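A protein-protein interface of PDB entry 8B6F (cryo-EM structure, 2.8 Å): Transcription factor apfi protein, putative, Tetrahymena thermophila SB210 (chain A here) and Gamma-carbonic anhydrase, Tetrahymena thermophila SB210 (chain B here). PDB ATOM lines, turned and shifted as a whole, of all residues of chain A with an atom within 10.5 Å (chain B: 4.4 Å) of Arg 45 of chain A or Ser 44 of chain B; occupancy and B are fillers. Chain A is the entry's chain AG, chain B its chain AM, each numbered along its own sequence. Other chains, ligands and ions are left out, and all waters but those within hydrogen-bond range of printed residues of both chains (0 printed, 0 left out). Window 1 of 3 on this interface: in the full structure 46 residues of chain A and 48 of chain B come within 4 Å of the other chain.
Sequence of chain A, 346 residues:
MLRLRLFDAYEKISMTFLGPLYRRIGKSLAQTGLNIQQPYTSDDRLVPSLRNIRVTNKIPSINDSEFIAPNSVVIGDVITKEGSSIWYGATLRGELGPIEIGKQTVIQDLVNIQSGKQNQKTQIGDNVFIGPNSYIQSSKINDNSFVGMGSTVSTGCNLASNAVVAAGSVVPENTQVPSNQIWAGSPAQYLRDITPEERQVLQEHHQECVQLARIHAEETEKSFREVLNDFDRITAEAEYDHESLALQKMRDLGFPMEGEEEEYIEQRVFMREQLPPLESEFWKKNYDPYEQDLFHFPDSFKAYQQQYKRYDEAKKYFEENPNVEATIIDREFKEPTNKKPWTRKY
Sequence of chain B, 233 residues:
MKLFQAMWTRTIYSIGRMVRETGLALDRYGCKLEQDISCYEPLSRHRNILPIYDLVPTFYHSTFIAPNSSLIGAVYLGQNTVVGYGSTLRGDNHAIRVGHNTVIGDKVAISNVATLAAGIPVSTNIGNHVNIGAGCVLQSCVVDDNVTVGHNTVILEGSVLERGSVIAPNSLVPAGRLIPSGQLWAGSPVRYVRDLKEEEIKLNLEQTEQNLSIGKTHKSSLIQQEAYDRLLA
Among the printed residues, pairs that only touch across the chains: Val 47 of chain A with Ser 44 of chain B (3.2 Å), Pro 48 of chain A with Pro 67 of chain B (3.7 Å), Arg 45 of chain A with Arg 47 of chain B (3.7 Å), Arg 45 of chain A with Ser 44 of chain B (3.8 Å), Leu 50 of chain A with Pro 67 of chain B (3.8 Å), Val 47 of chain A with His 46 of chain B (3.8 Å) and Asp 43 of chain A with Arg 47 of chain B (3.98 Å).
The backbone carbonyl oxygen of Ser 42 of chain A is in hydrogen-bond range of the guanidinium group of Arg 47 of chain B, at 2.8 Å. OD2 of Asp 44 of chain A is in salt-bridge range of NH2 of Arg 45 of chain B, at 3.5 Å. The guanidinium group (NH2) of Arg 47 of chain B is in salt-bridge range of the side-chain carboxylate (OD1) of Asp 44 of chain A (2.8 Å). The guanidinium group (NE) of Arg 45 of chain A sits at hydrogen-bond distance from the backbone carbonyl oxygen (O) of His 46 of chain B. NH2 of Arg 45 of chain A is in hydrogen-bond range of O of Pro 67 of chain B (3.2 Å). The guanidinium group (NE) of Arg 45 of chain A lies close to the backbone NH (N) of Asn 48 of chain B (3.3 Å).
Of chain B, only Ser 44 (3.8 Å), His 46 (3.2 Å), Arg 47 (3.7 Å), Asn 48 (3.3 Å) and Pro 67 (3.2 Å) come within 4 Å of Arg 45 of chain A. Of the printed residues of chain B, Val 47 of chain A touches Ser 44 (3.2 Å) and His 46 (3.8 Å). Of the printed residues of chain B, Pro 48 of chain A touches Pro 67. Of chain A, only Arg 45 and Val 47 come within 4 Å of Ser 44 of chain B. Of chain A, only Arg 45 and Val 47 come within 4 Å of His 46 of chain B. Printed residues of chain A within 4 Å of Arg 47 of chain B: Ser 42 (2.8 Å), Asp 43 (3.98 Å), Asp 44 (2.8 Å) and Arg 45 (3.7 Å). Of the printed residues of chain A, Pro 67 of chain B touches Arg 45, Pro 48 and Leu 50. The nearest residue of chain A that does not touch Ser 44 of chain B is Asp 44 of chain A (5.4 Å).
Of the 7 printed residues of chain B, 6 touch a printed residue of chain A. Hydrophobic or aromatic side chains of chain B within 4 Å of the printed part of chain A: His 46 and Pro 67. Among the printed residues, 13 pairs touch across the chains. Among the printed residues, Asp or Glu carboxylates within 4 Å of a Lys or Arg side-chain nitrogen of the other chain: Asp 44 of chain A with Arg 45 of chain B (3.5 Å) and Asp 44 of chain A with Arg 47 of chain B (2.8 Å).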
ATOM      1  N   LEU A  34     -35.727 -17.300 -21.109  1.00  0.00           N
ATOM      2  CA  LEU A  34     -34.387 -17.461 -21.663  1.00  0.00           C
ATOM      3  C   LEU A  34     -34.178 -18.880 -22.174  1.00  0.00           C
ATOM      4  O   LEU A  34     -33.630 -19.080 -23.263  1.00  0.00           O
ATOM      5  CB  LEU A  34     -33.339 -17.102 -20.609  1.00  0.00           C
ATOM      6  CG  LEU A  34     -31.879 -17.126 -21.066  1.00  0.00           C
ATOM      7  CD1 LEU A  34     -31.633 -16.100 -22.160  1.00  0.00           C
ATOM      8  CD2 LEU A  34     -30.954 -16.882 -19.889  1.00  0.00           C
ATOM      9  N   SER A  42     -28.890 -14.167 -26.390  1.00  0.00           N
ATOM     10  CA  SER A  42     -27.824 -13.949 -25.426  1.00  0.00           C
ATOM     11  C   SER A  42     -28.369 -13.138 -24.262  1.00  0.00           C
ATOM     12  O   SER A  42     -29.259 -12.302 -24.430  1.00  0.00           O
ATOM     13  CB  SER A  42     -26.625 -13.230 -26.037  1.00  0.00           C
ATOM     14  OG  SER A  42     -27.019 -12.040 -26.693  1.00  0.00           O
ATOM     15  N   ASP A  43     -27.829 -13.400 -23.078  1.00  0.00           N
ATOM     16  CA  ASP A  43     -28.237 -12.721 -21.861  1.00  0.00           C
ATOM     17  C   ASP A  43     -27.107 -11.824 -21.368  1.00  0.00           C
ATOM     18  O   ASP A  43     -25.943 -11.991 -21.741  1.00  0.00           O
ATOM     19  CB  ASP A  43     -28.624 -13.734 -20.778  1.00  0.00           C
ATOM     20  CG  ASP A  43     -29.307 -13.088 -19.592  1.00  0.00           C
ATOM     21  OD1 ASP A  43     -30.404 -12.521 -19.773  1.00  0.00           O
ATOM     22  OD2 ASP A  43     -28.750 -13.151 -18.477  1.00  0.00           O
ATOM     23  N   ASP A  44     -27.470 -10.862 -20.527  1.00  0.00           N
ATOM     24  CA  ASP A  44     -26.483  -9.943 -19.979  1.00  0.00           C
ATOM     25  C   ASP A  44     -25.496 -10.694 -19.092  1.00  0.00           C
ATOM     26  O   ASP A  44     -25.823 -11.713 -18.481  1.00  0.00           O
ATOM     27  CB  ASP A  44     -27.171  -8.838 -19.178  1.00  0.00           C
ATOM     28  CG  ASP A  44     -28.180  -8.066 -20.004  1.00  0.00           C
ATOM     29  OD1 ASP A  44     -27.922  -7.839 -21.203  1.00  0.00           O
ATOM     30  OD2 ASP A  44     -29.235  -7.692 -19.455  1.00  0.00           O
ATOM     31  N   ARG A  45     -24.274 -10.175 -19.030  1.00  0.00           N
ATOM     32  CA  ARG A  45     -23.193 -10.800 -18.284  1.00  0.00           C
ATOM     33  C   ARG A  45     -22.491  -9.753 -17.433  1.00  0.00           C
ATOM     34  O   ARG A  45     -22.617  -8.548 -17.660  1.00  0.00           O
ATOM     35  CB  ARG A  45     -22.179 -11.471 -19.220  1.00  0.00           C
ATOM     36  CG  ARG A  45     -21.312 -10.483 -19.986  1.00  0.00           C
ATOM     37  CD  ARG A  45     -20.549 -11.164 -21.107  1.00  0.00           C
ATOM     38  NE  ARG A  45     -19.697 -10.229 -21.832  1.00  0.00           N
ATOM     39  CZ  ARG A  45     -18.414 -10.014 -21.574  1.00  0.00           C
ATOM     40  NH1 ARG A  45     -17.787 -10.654 -20.601  1.00  0.00           N
ATOM     41  NH2 ARG A  45     -17.743  -9.136 -22.311  1.00  0.00           N
ATOM     42  N   LEU A  46     -21.752 -10.233 -16.438  1.00  0.00           N
ATOM     43  CA  LEU A  46     -20.907  -9.372 -15.616  1.00  0.00           C
ATOM     44  C   LEU A  46     -19.581  -9.199 -16.342  1.00  0.00           C
ATOM     45  O   LEU A  46     -18.735 -10.094 -16.338  1.00  0.00           O
ATOM     46  CB  LEU A  46     -20.714  -9.972 -14.230  1.00  0.00           C
ATOM     47  CG  LEU A  46     -22.000 -10.266 -13.456  1.00  0.00           C
ATOM     48  CD1 LEU A  46     -21.686 -10.927 -12.127  1.00  0.00           C
ATOM     49  CD2 LEU A  46     -22.805  -8.998 -13.241  1.00  0.00           C
ATOM     50  N   VAL A  47     -19.399  -8.049 -16.976  1.00  0.00           N
ATOM     51  CA  VAL A  47     -18.192  -7.829 -17.779  1.00  0.00           C
ATOM     52  C   VAL A  47     -16.977  -7.821 -16.858  1.00  0.00           C
ATOM     53  O   VAL A  47     -16.960  -7.065 -15.870  1.00  0.00           O
ATOM     54  CB  VAL A  47     -18.304  -6.515 -18.557  1.00  0.00           C
ATOM     55  CG1 VAL A  47     -17.050  -6.272 -19.385  1.00  0.00           C
ATOM     56  CG2 VAL A  47     -19.534  -6.525 -19.447  1.00  0.00           C
ATOM     57  N   PRO A  48     -15.950  -8.626 -17.122  1.00  0.00           N
ATOM     58  CA  PRO A  48     -14.777  -8.619 -16.244  1.00  0.00           C
ATOM     59  C   PRO A  48     -14.004  -7.316 -16.349  1.00  0.00           C
ATOM     60  O   PRO A  48     -13.969  -6.667 -17.396  1.00  0.00           O
ATOM     61  CB  PRO A  48     -13.946  -9.800 -16.756  1.00  0.00           C
ATOM     62  CG  PRO A  48     -14.334  -9.934 -18.178  1.00  0.00           C
ATOM     63  CD  PRO A  48     -15.785  -9.561 -18.248  1.00  0.00           C
ATOM     64  N   SER A  49     -13.374  -6.936 -15.241  1.00  0.00           N
ATOM     65  CA  SER A  49     -12.502  -5.768 -15.206  1.00  0.00           C
ATOM     66  C   SER A  49     -11.098  -6.204 -15.606  1.00  0.00           C
ATOM     67  O   SER A  49     -10.445  -6.962 -14.882  1.00  0.00           O
ATOM     68  CB  SER A  49     -12.505  -5.135 -13.817  1.00  0.00           C
ATOM     69  OG  SER A  49     -11.608  -4.040 -13.753  1.00  0.00           O
ATOM     70  N   LEU A  50     -10.633  -5.726 -16.758  1.00  0.00           N
ATOM     71  CA  LEU A  50      -9.347  -6.139 -17.298  1.00  0.00           C
ATOM     72  C   LEU A  50      -8.207  -5.225 -16.876  1.00  0.00           C
ATOM     73  O   LEU A  50      -7.082  -5.403 -17.353  1.00  0.00           O
ATOM     74  CB  LEU A  50      -9.423  -6.216 -18.823  1.00  0.00           C
ATOM     75  CG  LEU A  50     -10.492  -7.176 -19.358  1.00  0.00           C
ATOM     76  CD1 LEU A  50     -10.451  -7.216 -20.865  1.00  0.00           C
ATOM     77  CD2 LEU A  50     -10.326  -8.582 -18.789  1.00  0.00           C
ATOM     78  N   PRO A  70     -11.949   2.555 -16.887  1.00  0.00           N
ATOM     79  CA  PRO A  70     -12.481   1.255 -16.451  1.00  0.00           C
ATOM     80  C   PRO A  70     -12.423   0.180 -17.522  1.00  0.00           C
ATOM     81  O   PRO A  70     -12.281  -1.002 -17.187  1.00  0.00           O
ATOM     82  CB  PRO A  70     -13.926   1.584 -16.052  1.00  0.00           C
ATOM     83  CG  PRO A  70     -14.260   2.813 -16.808  1.00  0.00           C
ATOM     84  CD  PRO A  70     -12.991   3.597 -16.898  1.00  0.00           C
ATOM     85  N   ASN A  71     -12.531   0.547 -18.798  1.00  0.00           N
ATOM     86  CA  ASN A  71     -12.555  -0.419 -19.888  1.00  0.00           C
ATOM     87  C   ASN A  71     -11.199  -0.580 -20.566  1.00  0.00           C
ATOM     88  O   ASN A  71     -11.120  -1.206 -21.626  1.00  0.00           O
ATOM     89  CB  ASN A  71     -13.611  -0.024 -20.921  1.00  0.00           C
ATOM     90  CG  ASN A  71     -13.310   1.298 -21.589  1.00  0.00           C
ATOM     91  OD1 ASN A  71     -12.671   2.170 -21.006  1.00  0.00           O
ATOM     92  ND2 ASN A  71     -13.773   1.455 -22.821  1.00  0.00           N
ATOM     93  N   LEU B  43     -25.044  -1.478 -15.423  1.00  0.00           N
ATOM     94  CA  LEU B  43     -23.924  -2.375 -15.610  1.00  0.00           C
ATOM     95  C   LEU B  43     -23.756  -2.579 -17.103  1.00  0.00           C
ATOM     96  O   LEU B  43     -24.726  -2.495 -17.859  1.00  0.00           O
ATOM     97  CB  LEU B  43     -24.207  -3.701 -14.898  1.00  0.00           C
ATOM     98  CG  LEU B  43     -23.936  -3.701 -13.391  1.00  0.00           C
ATOM     99  CD1 LEU B  43     -24.865  -4.681 -12.694  1.00  0.00           C
ATOM    100  CD2 LEU B  43     -22.496  -4.050 -13.085  1.00  0.00           C
ATOM    101  N   SER B  44     -22.527  -2.838 -17.541  1.00  0.00           N
ATOM    102  CA  SER B  44     -22.308  -2.890 -18.975  1.00  0.00           C
ATOM    103  C   SER B  44     -23.164  -4.001 -19.554  1.00  0.00           C
ATOM    104  O   SER B  44     -23.246  -5.099 -19.001  1.00  0.00           O
ATOM    105  CB  SER B  44     -20.837  -3.136 -19.319  1.00  0.00           C
ATOM    106  OG  SER B  44     -20.112  -3.646 -18.217  1.00  0.00           O
ATOM    107  N   ARG B  45     -23.805  -3.708 -20.676  1.00  0.00           N
ATOM    108  CA  ARG B  45     -24.668  -4.673 -21.325  1.00  0.00           C
ATOM    109  C   ARG B  45     -23.902  -5.408 -22.406  1.00  0.00           C
ATOM    110  O   ARG B  45     -24.482  -6.218 -23.132  1.00  0.00           O
ATOM    111  CB  ARG B  45     -25.904  -3.975 -21.903  1.00  0.00           C
ATOM    112  CG  ARG B  45     -26.778  -3.356 -20.818  1.00  0.00           C
ATOM    113  CD  ARG B  45     -28.220  -3.163 -21.247  1.00  0.00           C
ATOM    114  NE  ARG B  45     -28.925  -4.432 -21.383  1.00  0.00           N
ATOM    115  CZ  ARG B  45     -30.139  -4.565 -21.897  1.00  0.00           C
ATOM    116  NH1 ARG B  45     -30.819  -3.521 -22.340  1.00  0.00           N
ATOM    117  NH2 ARG B  45     -30.686  -5.773 -21.961  1.00  0.00           N
ATOM    118  N   HIS B  46     -22.604  -5.126 -22.515  1.00  0.00           N
ATOM    119  CA  HIS B  46     -21.783  -5.700 -23.563  1.00  0.00           C
ATOM    120  C   HIS B  46     -21.768  -7.212 -23.460  1.00  0.00           C
ATOM    121  O   HIS B  46     -21.608  -7.775 -22.373  1.00  0.00           O
ATOM    122  CB  HIS B  46     -20.354  -5.180 -23.461  1.00  0.00           C
ATOM    123  CG  HIS B  46     -19.492  -5.591 -24.611  1.00  0.00           C
ATOM    124  ND1 HIS B  46     -18.279  -6.225 -24.439  1.00  0.00           N
ATOM    125  CD2 HIS B  46     -19.662  -5.461 -25.946  1.00  0.00           C
ATOM    126  CE1 HIS B  46     -17.741  -6.466 -25.619  1.00  0.00           C
ATOM    127  NE2 HIS B  46     -18.560  -6.015 -26.551  1.00  0.00           N
ATOM    128  N   ARG B  47     -21.933  -7.865 -24.597  1.00  0.00           N
ATOM    129  CA  ARG B  47     -21.940  -9.312 -24.683  1.00  0.00           C
ATOM    130  C   ARG B  47     -20.801  -9.707 -25.605  1.00  0.00           C
ATOM    131  O   ARG B  47     -20.722  -9.208 -26.732  1.00  0.00           O
ATOM    132  CB  ARG B  47     -23.290  -9.800 -25.206  1.00  0.00           C
ATOM    133  CG  ARG B  47     -24.450  -8.987 -24.642  1.00  0.00           C
ATOM    134  CD  ARG B  47     -25.802  -9.606 -24.930  1.00  0.00           C
ATOM    135  NE  ARG B  47     -26.868  -8.915 -24.214  1.00  0.00           N
ATOM    136  CZ  ARG B  47     -28.160  -9.039 -24.487  1.00  0.00           C
ATOM    137  NH1 ARG B  47     -28.587  -9.823 -25.464  1.00  0.00           N
ATOM    138  NH2 ARG B  47     -29.045  -8.363 -23.762  1.00  0.00           N
ATOM    139  N   ASN B  48     -19.912 -10.584 -25.139  1.00  0.00           N
ATOM    140  CA  ASN B  48     -18.762 -10.912 -25.970  1.00  0.00           C
ATOM    141  C   ASN B  48     -19.255 -11.591 -27.232  1.00  0.00           C
ATOM    142  O   ASN B  48     -18.821 -11.271 -28.344  1.00  0.00           O
ATOM    143  CB  ASN B  48     -17.766 -11.791 -25.217  1.00  0.00           C
ATOM    144  CG  ASN B  48     -16.499 -12.032 -26.013  1.00  0.00           C
ATOM    145  OD1 ASN B  48     -16.409 -11.654 -27.181  1.00  0.00           O
ATOM    146  ND2 ASN B  48     -15.510 -12.645 -25.384  1.00  0.00           N
ATOM    147  N   PRO B  67     -12.018 -11.497 -23.526  1.00  0.00           N
ATOM    148  CA  PRO B  67     -13.297 -11.002 -22.993  1.00  0.00           C
ATOM    149  C   PRO B  67     -13.607  -9.580 -23.413  1.00  0.00           C
ATOM    150  O   PRO B  67     -14.778  -9.185 -23.398  1.00  0.00           O
ATOM    151  CB  PRO B  67     -13.114 -11.117 -21.473  1.00  0.00           C
ATOM    152  CG  PRO B  67     -11.649 -11.089 -21.264  1.00  0.00           C
ATOM    153  CD  PRO B  67     -11.045 -11.768 -22.454  1.00  0.00           C
